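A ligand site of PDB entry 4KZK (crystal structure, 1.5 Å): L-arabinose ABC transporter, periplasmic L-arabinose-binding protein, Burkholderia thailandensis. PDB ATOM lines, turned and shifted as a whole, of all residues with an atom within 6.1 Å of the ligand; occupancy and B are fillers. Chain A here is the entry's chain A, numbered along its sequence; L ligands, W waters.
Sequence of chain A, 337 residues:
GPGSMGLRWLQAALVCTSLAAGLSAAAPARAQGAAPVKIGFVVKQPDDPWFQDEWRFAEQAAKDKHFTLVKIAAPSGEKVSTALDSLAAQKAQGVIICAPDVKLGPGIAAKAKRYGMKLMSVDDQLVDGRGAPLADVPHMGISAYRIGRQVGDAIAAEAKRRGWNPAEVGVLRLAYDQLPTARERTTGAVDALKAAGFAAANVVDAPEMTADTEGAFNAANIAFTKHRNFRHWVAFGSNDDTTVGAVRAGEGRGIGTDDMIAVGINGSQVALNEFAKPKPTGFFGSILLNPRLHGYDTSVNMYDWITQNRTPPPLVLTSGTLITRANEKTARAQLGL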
ATOM      1  N   LYS A  44       7.972 -36.379  20.146  1.00  0.00           N
ATOM      2  CA  LYS A  44       9.204 -37.134  20.035  1.00  0.00           C
ATOM      3  C   LYS A  44       9.525 -38.004  21.252  1.00  0.00           C
ATOM      4  O   LYS A  44      10.200 -39.033  21.116  1.00  0.00           O
ATOM      5  CB  LYS A  44      10.390 -36.206  19.748  1.00  0.00           C
ATOM      6  CG  LYS A  44      10.625 -35.139  20.786  1.00  0.00           C
ATOM      7  CD  LYS A  44      11.839 -34.253  20.487  1.00  0.00           C
ATOM      8  CE  LYS A  44      12.057 -33.282  21.637  1.00  0.00           C
ATOM      9  NZ  LYS A  44      13.239 -32.351  21.469  1.00  0.00           N
ATOM     10  N   GLN A  45       9.086 -37.595  22.444  1.00  0.00           N
ATOM     11  CA  GLN A  45       9.591 -38.163  23.711  1.00  0.00           C
ATOM     12  C   GLN A  45       8.485 -38.240  24.747  1.00  0.00           C
ATOM     13  O   GLN A  45       8.381 -37.352  25.618  1.00  0.00           O
ATOM     14  CB  GLN A  45      10.767 -37.366  24.265  1.00  0.00           C
ATOM     15  CG  GLN A  45      12.085 -37.680  23.568  1.00  0.00           C
ATOM     16  CD  GLN A  45      13.221 -36.830  24.100  1.00  0.00           C
ATOM     17  OE1 GLN A  45      13.419 -36.728  25.316  1.00  0.00           O
ATOM     18  NE2 GLN A  45      13.973 -36.191  23.209  1.00  0.00           N
ATOM     19  N   ASP A  48       9.125 -37.660  28.522  1.00  0.00           N
ATOM     20  CA  ASP A  48       9.401 -36.298  28.998  1.00  0.00           C
ATOM     21  C   ASP A  48       8.031 -35.713  29.379  1.00  0.00           C
ATOM     22  O   ASP A  48       7.148 -35.611  28.531  1.00  0.00           O
ATOM     23  CB  ASP A  48      10.048 -35.482  27.880  1.00  0.00           C
ATOM     24  CG  ASP A  48      10.141 -33.985  28.157  1.00  0.00           C
ATOM     25  OD1 ASP A  48       9.635 -33.525  29.200  1.00  0.00           O
ATOM     26  OD2 ASP A  48      10.696 -33.287  27.271  1.00  0.00           O
ATOM     27  N   TRP A  50       6.930 -32.874  29.863  1.00  0.00           N
ATOM     28  CA  TRP A  50       6.506 -31.731  29.038  1.00  0.00           C
ATOM     29  C   TRP A  50       5.503 -32.153  27.976  1.00  0.00           C
ATOM     30  O   TRP A  50       4.492 -31.467  27.752  1.00  0.00           O
ATOM     31  CB  TRP A  50       7.723 -31.023  28.414  1.00  0.00           C
ATOM     32  CG  TRP A  50       7.351 -29.964  27.466  1.00  0.00           C
ATOM     33  CD1 TRP A  50       7.403 -30.021  26.095  1.00  0.00           C
ATOM     34  CD2 TRP A  50       6.812 -28.701  27.792  1.00  0.00           C
ATOM     35  NE1 TRP A  50       6.941 -28.848  25.568  1.00  0.00           N
ATOM     36  CE2 TRP A  50       6.573 -28.018  26.587  1.00  0.00           C
ATOM     37  CE3 TRP A  50       6.479 -28.066  29.000  1.00  0.00           C
ATOM     38  CZ2 TRP A  50       6.024 -26.731  26.558  1.00  0.00           C
ATOM     39  CZ3 TRP A  50       5.955 -26.800  28.953  1.00  0.00           C
ATOM     40  CH2 TRP A  50       5.747 -26.138  27.742  1.00  0.00           C
ATOM     41  N   PHE A  51       5.770 -33.269  27.306  1.00  0.00           N
ATOM     42  CA  PHE A  51       4.900 -33.707  26.229  1.00  0.00           C
ATOM     43  C   PHE A  51       3.618 -34.309  26.772  1.00  0.00           C
ATOM     44  O   PHE A  51       2.564 -34.182  26.166  1.00  0.00           O
ATOM     45  CB  PHE A  51       5.653 -34.648  25.276  1.00  0.00           C
ATOM     46  CG  PHE A  51       6.708 -33.931  24.493  1.00  0.00           C
ATOM     47  CD1 PHE A  51       6.359 -32.983  23.567  1.00  0.00           C
ATOM     48  CD2 PHE A  51       8.047 -34.143  24.726  1.00  0.00           C
ATOM     49  CE1 PHE A  51       7.337 -32.257  22.913  1.00  0.00           C
ATOM     50  CE2 PHE A  51       9.022 -33.407  24.073  1.00  0.00           C
ATOM     51  CZ  PHE A  51       8.658 -32.486  23.148  1.00  0.00           C
ATOM     52  N   GLU A  54       1.635 -31.174  27.323  1.00  0.00           N
ATOM     53  CA  GLU A  54       1.025 -30.726  26.046  1.00  0.00           C
ATOM     54  C   GLU A  54      -0.204 -31.546  25.750  1.00  0.00           C
ATOM     55  O   GLU A  54      -1.248 -30.980  25.388  1.00  0.00           O
ATOM     56  CB  GLU A  54       2.031 -30.863  24.912  1.00  0.00           C
ATOM     57  CG  GLU A  54       3.075 -29.768  24.914  1.00  0.00           C
ATOM     58  CD  GLU A  54       3.993 -29.850  23.711  1.00  0.00           C
ATOM     59  OE1 GLU A  54       3.995 -30.873  23.022  1.00  0.00           O
ATOM     60  OE2 GLU A  54       4.742 -28.865  23.469  1.00  0.00           O
ATOM     61  N   CYS A  98       5.940 -32.548  17.253  1.00  0.00           N
ATOM     62  CA  CYS A  98       7.306 -32.241  17.659  1.00  0.00           C
ATOM     63  C   CYS A  98       8.130 -33.418  17.200  1.00  0.00           C
ATOM     64  O   CYS A  98       8.127 -34.459  17.845  1.00  0.00           O
ATOM     65  CB  CYS A  98       7.457 -32.036  19.167  1.00  0.00           C
ATOM     66  SG  CYS A  98       9.182 -31.596  19.583  1.00  0.00           S
ATOM     67  N   VAL A 122       5.356 -27.960  16.800  1.00  0.00           N
ATOM     68  CA  VAL A 122       5.450 -27.435  18.164  1.00  0.00           C
ATOM     69  C   VAL A 122       6.820 -27.808  18.714  1.00  0.00           C
ATOM     70  O   VAL A 122       7.319 -28.913  18.458  1.00  0.00           O
ATOM     71  CB  VAL A 122       4.263 -27.902  19.043  1.00  0.00           C
ATOM     72  CG1 VAL A 122       4.278 -29.401  19.276  1.00  0.00           C
ATOM     73  CG2 VAL A 122       4.198 -27.124  20.343  1.00  0.00           C
ATOM     74  N   ASP A 123       7.413 -26.864  19.449  1.00  0.00           N
ATOM     75  CA  ASP A 123       8.696 -26.966  20.136  1.00  0.00           C
ATOM     76  C   ASP A 123       9.886 -26.919  19.217  1.00  0.00           C
ATOM     77  O   ASP A 123      10.668 -25.989  19.297  1.00  0.00           O
ATOM     78  CB  ASP A 123       8.737 -28.189  21.053  1.00  0.00           C
ATOM     79  CG  ASP A 123       7.544 -28.245  21.957  1.00  0.00           C
ATOM     80  OD1 ASP A 123       7.364 -27.274  22.738  1.00  0.00           O
ATOM     81  OD2 ASP A 123       6.760 -29.196  21.872  1.00  0.00           O
ATOM     82  N   ASP A 124       9.991 -27.888  18.315  1.00  0.00           N
ATOM     83  CA  ASP A 124      11.150 -28.077  17.479  1.00  0.00           C
ATOM     84  C   ASP A 124      10.744 -27.803  16.040  1.00  0.00           C
ATOM     85  O   ASP A 124       9.989 -28.577  15.447  1.00  0.00           O
ATOM     86  CB  ASP A 124      11.710 -29.471  17.614  1.00  0.00           C
ATOM     87  CG  ASP A 124      12.157 -29.824  19.035  1.00  0.00           C
ATOM     88  OD1 ASP A 124      12.039 -28.966  19.937  1.00  0.00           O
ATOM     89  OD2 ASP A 124      12.624 -30.981  19.232  1.00  0.00           O
ATOM     90  N   MET A 140       4.965 -23.153  16.931  1.00  0.00           N
ATOM     91  CA  MET A 140       5.010 -22.554  18.254  1.00  0.00           C
ATOM     92  C   MET A 140       6.149 -23.165  19.025  1.00  0.00           C
ATOM     93  O   MET A 140       6.250 -24.400  19.104  1.00  0.00           O
ATOM     94  CB  MET A 140       3.718 -22.743  19.027  1.00  0.00           C
ATOM     95  CG  MET A 140       3.736 -22.038  20.369  1.00  0.00           C
ATOM     96  SD  MET A 140       2.282 -22.236  21.412  1.00  0.00           S
ATOM     97  CE  MET A 140       1.018 -21.455  20.415  1.00  0.00           C
ATOM     98  N   GLY A 141       7.035 -22.325  19.549  1.00  0.00           N
ATOM     99  CA  GLY A 141       8.116 -22.788  20.414  1.00  0.00           C
ATOM    100  C   GLY A 141       8.415 -21.753  21.454  1.00  0.00           C
ATOM    101  O   GLY A 141       7.643 -20.803  21.614  1.00  0.00           O
ATOM    102  N   ILE A 142       9.524 -21.927  22.153  1.00  0.00           N
ATOM    103  CA  ILE A 142       9.898 -20.993  23.192  1.00  0.00           C
ATOM    104  C   ILE A 142      10.869 -19.953  22.636  1.00  0.00           C
ATOM    105  O   ILE A 142      11.563 -20.217  21.650  1.00  0.00           O
ATOM    106  CB  ILE A 142      10.493 -21.687  24.435  1.00  0.00           C
ATOM    107  CG1 ILE A 142      11.903 -22.268  24.199  1.00  0.00           C
ATOM    108  CG2 ILE A 142       9.550 -22.761  24.916  1.00  0.00           C
ATOM    109  CD1 ILE A 142      12.543 -22.819  25.449  1.00  0.00           C
ATOM    110  N   LEU A 179      20.465 -29.191  17.242  1.00  0.00           N
ATOM    111  CA  LEU A 179      19.091 -28.682  17.244  1.00  0.00           C
ATOM    112  C   LEU A 179      19.083 -27.201  17.615  1.00  0.00           C
ATOM    113  O   LEU A 179      19.442 -26.859  18.728  1.00  0.00           O
ATOM    114  CB  LEU A 179      18.253 -29.471  18.232  1.00  0.00           C
ATOM    115  CG  LEU A 179      16.778 -29.069  18.369  1.00  0.00           C
ATOM    116  CD1 LEU A 179      16.003 -29.361  17.090  1.00  0.00           C
ATOM    117  CD2 LEU A 179      16.142 -29.733  19.573  1.00  0.00           C
ATOM    118  N   THR A 181      16.988 -24.903  18.687  1.00  0.00           N
ATOM    119  CA  THR A 181      16.396 -24.426  19.933  1.00  0.00           C
ATOM    120  C   THR A 181      17.272 -24.832  21.103  1.00  0.00           C
ATOM    121  O   THR A 181      17.430 -24.090  22.067  1.00  0.00           O
ATOM    122  CB  THR A 181      14.914 -24.845  20.121  1.00  0.00           C
ATOM    123  OG1 THR A 181      14.368 -24.213  21.281  1.00  0.00           O
ATOM    124  CG2 THR A 181      14.765 -26.354  20.244  1.00  0.00           C
ATOM    125  N   ARG A 185      19.243 -22.090  23.673  1.00  0.00           N
ATOM    126  CA  ARG A 185      19.039 -22.148  25.117  1.00  0.00           C
ATOM    127  C   ARG A 185      20.373 -22.142  25.848  1.00  0.00           C
ATOM    128  O   ARG A 185      20.532 -21.412  26.819  1.00  0.00           O
ATOM    129  CB  ARG A 185      18.270 -23.407  25.522  1.00  0.00           C
ATOM    130  CG  ARG A 185      16.854 -23.441  25.017  1.00  0.00           C
ATOM    131  CD  ARG A 185      16.238 -24.823  25.073  1.00  0.00           C
ATOM    132  NE  ARG A 185      15.127 -24.936  24.139  1.00  0.00           N
ATOM    133  CZ  ARG A 185      14.092 -25.773  24.293  1.00  0.00           C
ATOM    134  NH1 ARG A 185      14.032 -26.551  25.365  1.00  0.00           N
ATOM    135  NH2 ARG A 185      13.128 -25.838  23.376  1.00  0.00           N
ATOM    136  N   ALA A 211      19.631 -36.135  23.465  1.00  0.00           N
ATOM    137  CA  ALA A 211      19.182 -35.012  24.250  1.00  0.00           C
ATOM    138  C   ALA A 211      18.167 -35.516  25.283  1.00  0.00           C
ATOM    139  O   ALA A 211      16.947 -35.270  25.173  1.00  0.00           O
ATOM    140  CB  ALA A 211      18.545 -33.967  23.363  1.00  0.00           C
ATOM    141  N   SER A 238      19.368 -28.202  27.736  1.00  0.00           N
ATOM    142  CA  SER A 238      18.261 -27.755  26.923  1.00  0.00           C
ATOM    143  C   SER A 238      16.934 -27.856  27.664  1.00  0.00           C
ATOM    144  O   SER A 238      15.967 -27.218  27.280  1.00  0.00           O
ATOM    145  CB  SER A 238      18.205 -28.543  25.624  1.00  0.00           C
ATOM    146  OG  SER A 238      18.070 -29.925  25.870  1.00  0.00           O
ATOM    147  N   ASN A 239      16.887 -28.679  28.707  1.00  0.00           N
ATOM    148  CA  ASN A 239      15.656 -28.898  29.461  1.00  0.00           C
ATOM    149  C   ASN A 239      15.949 -29.488  30.825  1.00  0.00           C
ATOM    150  O   ASN A 239      17.107 -29.724  31.167  1.00  0.00           O
ATOM    151  CB  ASN A 239      14.643 -29.753  28.653  1.00  0.00           C
ATOM    152  CG  ASN A 239      15.097 -31.188  28.441  1.00  0.00           C
ATOM    153  OD1 ASN A 239      16.155 -31.600  28.879  1.00  0.00           O
ATOM    154  ND2 ASN A 239      14.274 -31.960  27.738  1.00  0.00           N
ATOM    155  N   ASP A 240      14.893 -29.705  31.615  1.00  0.00           N
ATOM    156  CA  ASP A 240      15.042 -30.318  32.938  1.00  0.00           C
ATOM    157  C   ASP A 240      15.690 -31.696  32.868  1.00  0.00           C
ATOM    158  O   ASP A 240      16.518 -32.042  33.723  1.00  0.00           O
ATOM    159  CB  ASP A 240      13.686 -30.437  33.654  1.00  0.00           C
ATOM    160  CG  ASP A 240      13.061 -29.100  34.002  1.00  0.00           C
ATOM    161  OD1 ASP A 240      13.799 -28.137  34.194  1.00  0.00           O
ATOM    162  OD2 ASP A 240      11.810 -29.024  34.120  1.00  0.00           O
ATOM    163  N   ASP A 241      15.286 -32.488  31.886  1.00  0.00           N
ATOM    164  CA  ASP A 241      15.753 -33.861  31.791  1.00  0.00           C
ATOM    165  C   ASP A 241      17.252 -33.962  31.629  1.00  0.00           C
ATOM    166  O   ASP A 241      17.915 -34.717  32.327  1.00  0.00           O
ATOM    167  CB  ASP A 241      15.061 -34.543  30.614  1.00  0.00           C
ATOM    168  CG  ASP A 241      13.533 -34.485  30.712  1.00  0.00           C
ATOM    169  OD1 ASP A 241      13.020 -33.468  31.178  1.00  0.00           O
ATOM    170  OD2 ASP A 241      12.884 -35.419  30.221  1.00  0.00           O
ATOM    171  N   ILE A 265      15.041 -26.115  32.168  1.00  0.00           N
ATOM    172  CA  ILE A 265      13.966 -25.493  31.398  1.00  0.00           C
ATOM    173  C   ILE A 265      12.815 -26.504  31.297  1.00  0.00           C
ATOM    174  O   ILE A 265      13.077 -27.671  30.980  1.00  0.00           O
ATOM    175  CB  ILE A 265      14.415 -25.069  29.997  1.00  0.00           C
ATOM    176  CG1 ILE A 265      15.508 -24.002  30.093  1.00  0.00           C
ATOM    177  CG2 ILE A 265      13.231 -24.584  29.179  1.00  0.00           C
ATOM    178  CD1 ILE A 265      16.227 -23.786  28.782  1.00  0.00           C
ATOM    179  N   ASN A 266      11.611 -26.036  31.626  1.00  0.00           N
ATOM    180  CA  ASN A 266      10.278 -26.651  31.445  1.00  0.00           C
ATOM    181  C   ASN A 266       9.426 -26.412  32.677  1.00  0.00           C
ATOM    182  O   ASN A 266       8.328 -25.944  32.575  1.00  0.00           O
ATOM    183  CB  ASN A 266      10.303 -28.137  31.144  1.00  0.00           C
ATOM    184  CG  ASN A 266      10.750 -28.462  29.759  1.00  0.00           C
ATOM    185  OD1 ASN A 266      10.839 -27.575  28.897  1.00  0.00           O
ATOM    186  ND2 ASN A 266      11.012 -29.744  29.500  1.00  0.00           N
ATOM    187  N   LEU A 289       7.826 -23.124  31.769  1.00  0.00           N
ATOM    188  CA  LEU A 289       7.114 -22.864  30.519  1.00  0.00           C
ATOM    189  C   LEU A 289       5.614 -23.112  30.657  1.00  0.00           C
ATOM    190  O   LEU A 289       5.121 -23.645  31.660  1.00  0.00           O
ATOM    191  CB  LEU A 289       7.681 -23.764  29.418  1.00  0.00           C
ATOM    192  CG  LEU A 289       9.188 -23.647  29.162  1.00  0.00           C
ATOM    193  CD1 LEU A 289       9.563 -24.612  28.057  1.00  0.00           C
ATOM    194  CD2 LEU A 289       9.673 -22.240  28.831  1.00  0.00           C
ATOM    195  N   HIS A 294       1.361 -24.359  24.351  1.00  0.00           N
ATOM    196  CA  HIS A 294       1.863 -25.355  23.399  1.00  0.00           C
ATOM    197  C   HIS A 294       0.930 -26.522  23.114  1.00  0.00           C
ATOM    198  O   HIS A 294       1.060 -27.166  22.085  1.00  0.00           O
ATOM    199  CB  HIS A 294       3.213 -25.887  23.891  1.00  0.00           C
ATOM    200  CG  HIS A 294       4.319 -24.879  23.826  1.00  0.00           C
ATOM    201  ND1 HIS A 294       5.584 -25.179  23.364  1.00  0.00           N
ATOM    202  CD2 HIS A 294       4.337 -23.566  24.174  1.00  0.00           C
ATOM    203  CE1 HIS A 294       6.338 -24.097  23.429  1.00  0.00           C
ATOM    204  NE2 HIS A 294       5.614 -23.101  23.908  1.00  0.00           N
HETATM  205  C1  LIG L   1      11.786 -29.449  23.314  1.00  0.00           C
HETATM  206  C2  LIG L   1      12.304 -30.218  24.524  1.00  0.00           C
HETATM  207  C3  LIG L   1      11.205 -30.223  25.602  1.00  0.00           C
HETATM  208  C4  LIG L   1      10.774 -28.791  25.897  1.00  0.00           C
HETATM  209  C5  LIG L   1      10.313 -28.140  24.601  1.00  0.00           C
HETATM  210  C6  LIG L   1       9.919 -26.684  24.817  1.00  0.00           C
HETATM  211  O1  LIG L   1      12.851 -29.348  22.390  1.00  0.00           O
HETATM  212  O2  LIG L   1      12.603 -31.529  24.108  1.00  0.00           O
HETATM  213  O3  LIG L   1      11.654 -30.885  26.794  1.00  0.00           O
HETATM  214  O4  LIG L   1      11.804 -28.063  26.504  1.00  0.00           O
HETATM  215  O5  LIG L   1      11.399 -28.131  23.693  1.00  0.00           O
HETATM  216  O6  LIG L   1       9.495 -26.086  23.606  1.00  0.00           O
HETATM  217  O   HOH W   1      15.510 -28.975  23.139  1.00  0.00           O
HETATM  218  O   HOH W   2      15.324 -33.059  24.430  1.00  0.00           O
HETATM  219  O   HOH W   3      10.773 -24.494  21.688  1.00  0.00           O
HETATM  220  O   HOH W   4      12.586 -33.826  25.471  1.00  0.00           O
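OD1 of Asp 123 is in hydrogen-bond range of O6 of the ligand (2.6 Å).
The side-chain carboxylate (OD1) of Asp 124 lies within hydrogen-bond range of an oxygen (O1) of the ligand, 2.6 Å away.
The side-chain amide oxygen (OD1) of Asn 266 lies within hydrogen-bond range of an oxygen (O4) of the ligand, at 2.6 Å.
The side-chain amino group (NZ) of Lys 44 lies within hydrogen-bond range of an oxygen (O2) of the ligand (2.8 Å).
An oxygen (O5) of the ligand is in hydrogen-bond range of the guanidinium group (NH2) of Arg 185 (2.9 Å).
The side-chain amide nitrogen (ND2) of Asn 239 is in hydrogen-bond range of an oxygen (O3) of the ligand (3.0 Å).
O3 of the ligand sits at hydrogen-bond distance from OD2 of Asp 48 (2.6 Å).
Trp 50 touches the ligand (NE1 to C5, 3.6 Å).
Ile 142 touches the ligand.
Leu 289 touches the ligand (CD1 to C6, 3.9 Å).
His 294 touches the ligand.
Hydrophobic or aromatic side chains within 4 Å of the ligand: Trp 50, Ile 142, Leu 289 and His 294.
Within 4 Å of the ligand: Lys 44, Asp 48, Trp 50, Asp 123, Asp 124, Ile 142, Arg 185, Asn 239, Asn 266, Leu 289 and His 294.
The nearest printed residue that does not touch the ligand is Phe 51 (4.04 Å).
Water W4 lies within hydrogen-bond range of the side-chain carboxylate (OD2) of Asp 48 (2.7 Å), an oxygen (O2) of the ligand (2.7 Å), the side-chain amide oxygen (OE1) of Gln 45 (3.0 Å) and the side-chain amide nitrogen (ND2) of Asn 239 (3.4 Å).
Water W3 lies within hydrogen-bond range of an oxygen (O6) of the ligand, the backbone carbonyl oxygen of Asp 123, the backbone NH of Ile 142 and the guanidinium group of Arg 185.
Water W2 bridges O of Ala 211 and O2 of the ligand.
The backbone NH (N) of Leu 289 is in hydrogen-bond range of the backbone carbonyl oxygen (O) of Asn 266, 3.0 Å away.
The side-chain amide oxygen (OD1) of Asn 239 sits close to the backbone NH (N) of Asp 241, at 3.3 Å.
OE2 of Glu 54 sits close to OD2 of Asp 123, 2.6 Å away.
The backbone NH (N) of Trp 50 lies within hydrogen-bond range of the side-chain carboxylate (OD1) of Asp 48 (2.9 Å).
The backbone NH of Lys 44 lies within hydrogen-bond range of the backbone carbonyl oxygen of Cys 98 (3.0 Å).
The side-chain carboxylate of Asp 123 sits at hydrogen-bond distance from the indole nitrogen of Trp 50, 3.3 Å away.
The backbone carbonyl oxygen (O) of Met 140 sits at hydrogen-bond distance from the backbone NH (N) of Asp 123, 2.7 Å away.
The side-chain hydroxyl (OG1) of Thr 181 lies within hydrogen-bond range of the guanidinium group (NH2) of Arg 185, 2.9 Å away.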
